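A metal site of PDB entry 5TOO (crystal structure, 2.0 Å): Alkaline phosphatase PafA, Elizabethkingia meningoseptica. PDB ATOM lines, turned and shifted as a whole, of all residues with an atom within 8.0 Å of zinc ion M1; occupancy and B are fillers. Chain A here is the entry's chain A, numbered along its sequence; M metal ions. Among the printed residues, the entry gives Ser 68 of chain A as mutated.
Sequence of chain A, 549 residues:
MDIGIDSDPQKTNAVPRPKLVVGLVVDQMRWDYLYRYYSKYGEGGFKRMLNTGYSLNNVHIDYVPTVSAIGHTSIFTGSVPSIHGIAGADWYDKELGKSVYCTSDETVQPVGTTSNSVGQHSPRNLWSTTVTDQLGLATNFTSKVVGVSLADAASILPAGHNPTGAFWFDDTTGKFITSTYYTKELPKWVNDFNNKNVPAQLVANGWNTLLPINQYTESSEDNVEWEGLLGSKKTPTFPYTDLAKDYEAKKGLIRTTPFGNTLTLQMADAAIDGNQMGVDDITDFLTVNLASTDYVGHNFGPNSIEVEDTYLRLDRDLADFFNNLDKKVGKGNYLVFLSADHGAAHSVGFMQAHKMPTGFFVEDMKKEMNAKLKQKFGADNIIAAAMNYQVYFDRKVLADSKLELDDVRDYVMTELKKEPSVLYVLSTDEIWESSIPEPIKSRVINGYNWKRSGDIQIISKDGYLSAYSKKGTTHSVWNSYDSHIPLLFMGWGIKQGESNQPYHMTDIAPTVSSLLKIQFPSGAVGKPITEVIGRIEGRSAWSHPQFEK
The backbone NH (N) of Asp 294 sits at hydrogen-bond distance from the backbone carbonyl oxygen (O) of Asp 27.
O of Leu 290 is in hydrogen-bond range of N of Asp 27.
The backbone carbonyl oxygen (O) of Asp 27 sits at hydrogen-bond distance from the side-chain hydroxyl (OG1) of Thr 293 (2.8 Å).
ND1 of His 475 sits close to ND1 of His 342, at 3.3 Å.
The backbone NH of Met 29 is in hydrogen-bond range of the backbone carbonyl oxygen of His 342, at 3.4 Å.
ND1 of His 72 sits close to OD2 of Asp 341.
The side-chain carboxylate (OD1) of Asp 341 is in hydrogen-bond range of the backbone NH (N) of Gln 28 (3.2 Å).
The backbone carbonyl oxygen (O) of Asp 294 sits at hydrogen-bond distance from the side-chain amide nitrogen (NE2) of Gln 28 (3.0 Å).
OD1 of Asp 294 touches zinc ion M1, 3.9 Å away.
Four residues have an atom within 4 Å of zinc ion M1: Asp 27, Asp 294, Asp 341 and His 342.
Zinc ion M1 is bound by OD1 of Asp 27, 2.0 Å away.
NE2 of His 342 binds zinc ion M1 (2.1 Å).
OD2 of Asp 341 is bound to zinc ion M1.
Zinc ion M1 has three donor atoms within binding distance.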
ATOM      1  N   VAL A  25       0.921  12.826   4.167  1.00  0.00           N
ATOM      2  CA  VAL A  25      -0.357  13.514   4.168  1.00  0.00           C
ATOM      3  C   VAL A  25      -0.391  14.415   5.377  1.00  0.00           C
ATOM      4  O   VAL A  25      -0.243  13.942   6.510  1.00  0.00           O
ATOM      5  CB  VAL A  25      -1.556  12.557   4.170  1.00  0.00           C
ATOM      6  CG1 VAL A  25      -2.842  13.365   4.115  1.00  0.00           C
ATOM      7  CG2 VAL A  25      -1.473  11.569   3.002  1.00  0.00           C
ATOM      8  N   VAL A  26      -0.586  15.702   5.132  1.00  0.00           N
ATOM      9  CA  VAL A  26      -0.732  16.697   6.162  1.00  0.00           C
ATOM     10  C   VAL A  26      -2.220  16.940   6.326  1.00  0.00           C
ATOM     11  O   VAL A  26      -2.873  17.532   5.475  1.00  0.00           O
ATOM     12  CB  VAL A  26       0.007  17.995   5.825  1.00  0.00           C
ATOM     13  CG1 VAL A  26      -0.092  18.960   7.027  1.00  0.00           C
ATOM     14  CG2 VAL A  26       1.469  17.694   5.442  1.00  0.00           C
ATOM     15  N   ASP A  27      -2.754  16.412   7.409  1.00  0.00           N
ATOM     16  CA  ASP A  27      -4.179  16.371   7.607  1.00  0.00           C
ATOM     17  C   ASP A  27      -4.758  17.776   7.765  1.00  0.00           C
ATOM     18  O   ASP A  27      -4.225  18.607   8.505  1.00  0.00           O
ATOM     19  CB  ASP A  27      -4.469  15.491   8.830  1.00  0.00           C
ATOM     20  CG  ASP A  27      -5.814  14.869   8.784  1.00  0.00           C
ATOM     21  OD1 ASP A  27      -6.781  15.594   8.552  1.00  0.00           O
ATOM     22  OD2 ASP A  27      -5.901  13.634   9.010  1.00  0.00           O
ATOM     23  N   GLN A  28      -5.830  18.075   7.032  1.00  0.00           N
ATOM     24  CA  GLN A  28      -6.494  19.384   7.058  1.00  0.00           C
ATOM     25  C   GLN A  28      -5.651  20.515   6.462  1.00  0.00           C
ATOM     26  O   GLN A  28      -6.027  21.701   6.608  1.00  0.00           O
ATOM     27  CB  GLN A  28      -6.914  19.757   8.484  1.00  0.00           C
ATOM     28  CG  GLN A  28      -8.117  20.671   8.562  1.00  0.00           C
ATOM     29  CD  GLN A  28      -8.393  21.221   9.996  1.00  0.00           C
ATOM     30  OE1 GLN A  28      -8.241  22.413  10.247  1.00  0.00           O
ATOM     31  NE2 GLN A  28      -8.823  20.336  10.921  1.00  0.00           N
ATOM     32  N   MET A  29      -4.563  20.209   5.756  1.00  0.00           N
ATOM     33  CA  MET A  29      -3.741  21.254   5.149  1.00  0.00           C
ATOM     34  C   MET A  29      -4.416  21.820   3.899  1.00  0.00           C
ATOM     35  O   MET A  29      -4.389  21.218   2.824  1.00  0.00           O
ATOM     36  CB  MET A  29      -2.362  20.730   4.812  1.00  0.00           C
ATOM     37  CG  MET A  29      -1.489  21.819   4.272  1.00  0.00           C
ATOM     38  SD  MET A  29       0.173  21.349   3.921  1.00  0.00           S
ATOM     39  CE  MET A  29       0.666  22.887   3.171  1.00  0.00           C
ATOM     40  N   THR A  66     -16.018  15.631   2.355  1.00  0.00           N
ATOM     41  CA  THR A  66     -14.568  15.687   2.553  1.00  0.00           C
ATOM     42  C   THR A  66     -14.223  15.506   4.028  1.00  0.00           C
ATOM     43  O   THR A  66     -13.618  16.376   4.685  1.00  0.00           O
ATOM     44  CB  THR A  66     -14.024  17.013   2.020  1.00  0.00           C
ATOM     45  OG1 THR A  66     -14.833  18.093   2.504  1.00  0.00           O
ATOM     46  CG2 THR A  66     -14.047  17.029   0.438  1.00  0.00           C
ATOM     47  N   VAL A  67     -14.600  14.344   4.558  1.00  0.00           N
ATOM     48  CA  VAL A  67     -14.346  14.036   5.962  1.00  0.00           C
ATOM     49  C   VAL A  67     -13.107  13.157   6.116  1.00  0.00           C
ATOM     50  O   VAL A  67     -12.388  12.866   5.166  1.00  0.00           O
ATOM     51  CB  VAL A  67     -15.557  13.370   6.628  1.00  0.00           C
ATOM     52  CG1 VAL A  67     -16.757  14.332   6.618  1.00  0.00           C
ATOM     53  CG2 VAL A  67     -15.924  12.062   5.930  1.00  0.00           C
ATOM     54  N   SER A  68     -12.891  12.740   7.358  1.00  0.00           N
ATOM     55  CA  SER A  68     -11.806  11.869   7.733  1.00  0.00           C
ATOM     56  C   SER A  68     -11.917  10.499   7.070  1.00  0.00           C
ATOM     57  O   SER A  68     -12.992  10.080   6.636  1.00  0.00           O
ATOM     58  CB  SER A  68     -11.844  11.668   9.253  1.00  0.00           C
ATOM     59  OG  SER A  68     -12.172  12.905   9.870  1.00  0.00           O
ATOM     60  N   ALA A  69     -10.785   9.799   7.042  1.00  0.00           N
ATOM     61  CA  ALA A  69     -10.669   8.433   6.527  1.00  0.00           C
ATOM     62  C   ALA A  69     -10.773   8.373   5.000  1.00  0.00           C
ATOM     63  O   ALA A  69      -9.952   7.723   4.368  1.00  0.00           O
ATOM     64  CB  ALA A  69     -11.718   7.515   7.157  1.00  0.00           C
ATOM     65  N   ILE A  70     -11.738   9.059   4.401  1.00  0.00           N
ATOM     66  CA  ILE A  70     -11.936   8.955   2.952  1.00  0.00           C
ATOM     67  C   ILE A  70     -10.740   9.548   2.199  1.00  0.00           C
ATOM     68  O   ILE A  70     -10.242   8.961   1.230  1.00  0.00           O
ATOM     69  CB  ILE A  70     -13.236   9.642   2.506  1.00  0.00           C
ATOM     70  CG1 ILE A  70     -14.450   9.225   3.337  1.00  0.00           C
ATOM     71  CG2 ILE A  70     -13.507   9.360   1.033  1.00  0.00           C
ATOM     72  CD1 ILE A  70     -15.788   9.983   2.908  1.00  0.00           C
ATOM     73  N   GLY A  71     -10.307  10.744   2.600  1.00  0.00           N
ATOM     74  CA  GLY A  71      -9.207  11.385   1.902  1.00  0.00           C
ATOM     75  C   GLY A  71      -7.959  10.527   1.885  1.00  0.00           C
ATOM     76  O   GLY A  71      -7.298  10.395   0.860  1.00  0.00           O
ATOM     77  N   HIS A  72      -7.611   9.950   3.043  1.00  0.00           N
ATOM     78  CA  HIS A  72      -6.497   9.039   3.106  1.00  0.00           C
ATOM     79  C   HIS A  72      -6.740   7.839   2.203  1.00  0.00           C
ATOM     80  O   HIS A  72      -5.891   7.486   1.377  1.00  0.00           O
ATOM     81  CB  HIS A  72      -6.253   8.604   4.572  1.00  0.00           C
ATOM     82  CG  HIS A  72      -5.765   9.732   5.426  1.00  0.00           C
ATOM     83  ND1 HIS A  72      -6.576  10.448   6.275  1.00  0.00           N
ATOM     84  CD2 HIS A  72      -4.536  10.300   5.501  1.00  0.00           C
ATOM     85  CE1 HIS A  72      -5.869  11.407   6.850  1.00  0.00           C
ATOM     86  NE2 HIS A  72      -4.625  11.335   6.400  1.00  0.00           N
ATOM     87  N   ALA A 154      -5.610   6.807   9.533  1.00  0.00           N
ATOM     88  CA  ALA A 154      -4.617   7.447   8.689  1.00  0.00           C
ATOM     89  C   ALA A 154      -3.314   6.663   8.603  1.00  0.00           C
ATOM     90  O   ALA A 154      -2.476   6.967   7.741  1.00  0.00           O
ATOM     91  CB  ALA A 154      -4.374   8.871   9.229  1.00  0.00           C
ATOM     92  N   ASN A 289       1.015  10.128   7.966  1.00  0.00           N
ATOM     93  CA  ASN A 289      -0.003  11.154   8.122  1.00  0.00           C
ATOM     94  C   ASN A 289       0.406  12.023   9.294  1.00  0.00           C
ATOM     95  O   ASN A 289       0.741  11.512  10.364  1.00  0.00           O
ATOM     96  CB  ASN A 289      -1.386  10.553   8.377  1.00  0.00           C
ATOM     97  CG  ASN A 289      -2.429  11.608   8.776  1.00  0.00           C
ATOM     98  OD1 ASN A 289      -2.707  12.519   8.013  1.00  0.00           O
ATOM     99  ND2 ASN A 289      -2.987  11.489   9.969  1.00  0.00           N
ATOM    100  N   LEU A 290       0.409  13.331   9.082  1.00  0.00           N
ATOM    101  CA  LEU A 290       0.690  14.318  10.120  1.00  0.00           C
ATOM    102  C   LEU A 290      -0.658  14.780  10.650  1.00  0.00           C
ATOM    103  O   LEU A 290      -1.269  15.691  10.082  1.00  0.00           O
ATOM    104  CB  LEU A 290       1.515  15.484   9.571  1.00  0.00           C
ATOM    105  CG  LEU A 290       2.996  15.279   9.202  1.00  0.00           C
ATOM    106  CD1 LEU A 290       3.759  14.505  10.244  1.00  0.00           C
ATOM    107  CD2 LEU A 290       3.250  14.600   7.899  1.00  0.00           C
ATOM    108  N   ALA A 291      -1.115  14.190  11.747  1.00  0.00           N
ATOM    109  CA  ALA A 291      -2.490  14.413  12.201  1.00  0.00           C
ATOM    110  C   ALA A 291      -2.681  15.708  12.977  1.00  0.00           C
ATOM    111  O   ALA A 291      -3.817  16.170  13.084  1.00  0.00           O
ATOM    112  CB  ALA A 291      -2.950  13.250  13.076  1.00  0.00           C
ATOM    113  N   THR A 293      -1.979  18.840  12.567  1.00  0.00           N
ATOM    114  CA  THR A 293      -2.574  19.989  11.851  1.00  0.00           C
ATOM    115  C   THR A 293      -4.095  19.948  11.909  1.00  0.00           C
ATOM    116  O   THR A 293      -4.763  20.989  11.943  1.00  0.00           O
ATOM    117  CB  THR A 293      -2.096  20.010  10.394  1.00  0.00           C
ATOM    118  OG1 THR A 293      -1.859  18.653   9.935  1.00  0.00           O
ATOM    119  CG2 THR A 293      -0.809  20.775  10.274  1.00  0.00           C
ATOM    120  N   ASP A 294      -4.668  18.750  11.916  1.00  0.00           N
ATOM    121  CA  ASP A 294      -6.118  18.619  11.973  1.00  0.00           C
ATOM    122  C   ASP A 294      -6.648  18.901  13.374  1.00  0.00           C
ATOM    123  O   ASP A 294      -7.524  19.759  13.551  1.00  0.00           O
ATOM    124  CB  ASP A 294      -6.501  17.220  11.499  1.00  0.00           C
ATOM    125  CG  ASP A 294      -7.970  16.976  11.526  1.00  0.00           C
ATOM    126  OD1 ASP A 294      -8.693  17.445  10.608  1.00  0.00           O
ATOM    127  OD2 ASP A 294      -8.392  16.291  12.460  1.00  0.00           O
ATOM    128  N   TYR A 295      -6.134  18.185  14.367  1.00  0.00           N
ATOM    129  CA  TYR A 295      -6.511  18.451  15.753  1.00  0.00           C
ATOM    130  C   TYR A 295      -6.418  19.932  16.100  1.00  0.00           C
ATOM    131  O   TYR A 295      -7.364  20.517  16.610  1.00  0.00           O
ATOM    132  CB  TYR A 295      -5.618  17.640  16.687  1.00  0.00           C
ATOM    133  CG  TYR A 295      -5.995  16.211  16.682  1.00  0.00           C
ATOM    134  CD1 TYR A 295      -7.056  15.760  17.450  1.00  0.00           C
ATOM    135  CD2 TYR A 295      -5.291  15.302  15.905  1.00  0.00           C
ATOM    136  CE1 TYR A 295      -7.392  14.429  17.463  1.00  0.00           C
ATOM    137  CE2 TYR A 295      -5.616  13.981  15.894  1.00  0.00           C
ATOM    138  CZ  TYR A 295      -6.681  13.541  16.656  1.00  0.00           C
ATOM    139  OH  TYR A 295      -6.999  12.200  16.648  1.00  0.00           O
ATOM    140  N   HIS A 298      -8.952  21.776  14.093  1.00  0.00           N
ATOM    141  CA  HIS A 298     -10.316  21.598  14.585  1.00  0.00           C
ATOM    142  C   HIS A 298     -10.586  22.484  15.787  1.00  0.00           C
ATOM    143  O   HIS A 298     -11.719  22.936  15.967  1.00  0.00           O
ATOM    144  CB  HIS A 298     -10.575  20.136  14.953  1.00  0.00           C
ATOM    145  CG  HIS A 298     -11.037  19.308  13.788  1.00  0.00           C
ATOM    146  ND1 HIS A 298     -12.246  19.522  13.172  1.00  0.00           N
ATOM    147  CD2 HIS A 298     -10.443  18.299  13.125  1.00  0.00           C
ATOM    148  CE1 HIS A 298     -12.379  18.661  12.173  1.00  0.00           C
ATOM    149  NE2 HIS A 298     -11.295  17.916  12.121  1.00  0.00           N
ATOM    150  N   ALA A 340      -2.796  16.517   1.113  1.00  0.00           N
ATOM    151  CA  ALA A 340      -3.705  16.632   2.234  1.00  0.00           C
ATOM    152  C   ALA A 340      -4.923  15.796   1.923  1.00  0.00           C
ATOM    153  O   ALA A 340      -5.232  15.552   0.765  1.00  0.00           O
ATOM    154  CB  ALA A 340      -4.145  18.070   2.490  1.00  0.00           C
ATOM    155  N   ASP A 341      -5.646  15.397   2.972  1.00  0.00           N
ATOM    156  CA  ASP A 341      -6.858  14.598   2.829  1.00  0.00           C
ATOM    157  C   ASP A 341      -8.098  15.477   2.783  1.00  0.00           C
ATOM    158  O   ASP A 341      -9.199  14.974   2.546  1.00  0.00           O
ATOM    159  CB  ASP A 341      -6.940  13.594   3.972  1.00  0.00           C
ATOM    160  CG  ASP A 341      -7.074  14.258   5.338  1.00  0.00           C
ATOM    161  OD1 ASP A 341      -6.575  15.383   5.525  1.00  0.00           O
ATOM    162  OD2 ASP A 341      -7.705  13.641   6.220  1.00  0.00           O
ATOM    163  N   HIS A 342      -7.918  16.776   2.982  1.00  0.00           N
ATOM    164  CA  HIS A 342      -8.963  17.794   2.929  1.00  0.00           C
ATOM    165  C   HIS A 342      -8.396  19.108   3.427  1.00  0.00           C
ATOM    166  O   HIS A 342      -7.310  19.140   4.021  1.00  0.00           O
ATOM    167  CB  HIS A 342     -10.187  17.424   3.774  1.00  0.00           C
ATOM    168  CG  HIS A 342      -9.866  17.141   5.213  1.00  0.00           C
ATOM    169  ND1 HIS A 342      -9.696  18.137   6.141  1.00  0.00           N
ATOM    170  CD2 HIS A 342      -9.661  15.969   5.869  1.00  0.00           C
ATOM    171  CE1 HIS A 342      -9.407  17.595   7.318  1.00  0.00           C
ATOM    172  NE2 HIS A 342      -9.391  16.286   7.187  1.00  0.00           N
ATOM    173  N   GLY A 343      -9.117  20.189   3.174  1.00  0.00           N
ATOM    174  CA  GLY A 343      -8.806  21.507   3.689  1.00  0.00           C
ATOM    175  C   GLY A 343      -9.625  21.773   4.940  1.00  0.00           C
ATOM    176  O   GLY A 343      -9.817  20.879   5.778  1.00  0.00           O
ATOM    177  N   HIS A 475     -14.466  20.324   8.362  1.00  0.00           N
ATOM    178  CA  HIS A 475     -14.363  20.065   6.934  1.00  0.00           C
ATOM    179  C   HIS A 475     -15.419  19.043   6.578  1.00  0.00           C
ATOM    180  O   HIS A 475     -15.608  18.080   7.323  1.00  0.00           O
ATOM    181  CB  HIS A 475     -12.981  19.499   6.597  1.00  0.00           C
ATOM    182  CG  HIS A 475     -12.545  18.410   7.535  1.00  0.00           C
ATOM    183  ND1 HIS A 475     -12.648  17.066   7.223  1.00  0.00           N
ATOM    184  CD2 HIS A 475     -12.024  18.471   8.783  1.00  0.00           C
ATOM    185  CE1 HIS A 475     -12.183  16.354   8.234  1.00  0.00           C
ATOM    186  NE2 HIS A 475     -11.813  17.181   9.194  1.00  0.00           N
HETATM  187 ZN    ZN M   1      -8.411  14.643   7.940  1.00  0.00          ZN
HETATM  188 ZN    ZN M   2     -10.578  16.559  10.817  1.00  0.00          ZN
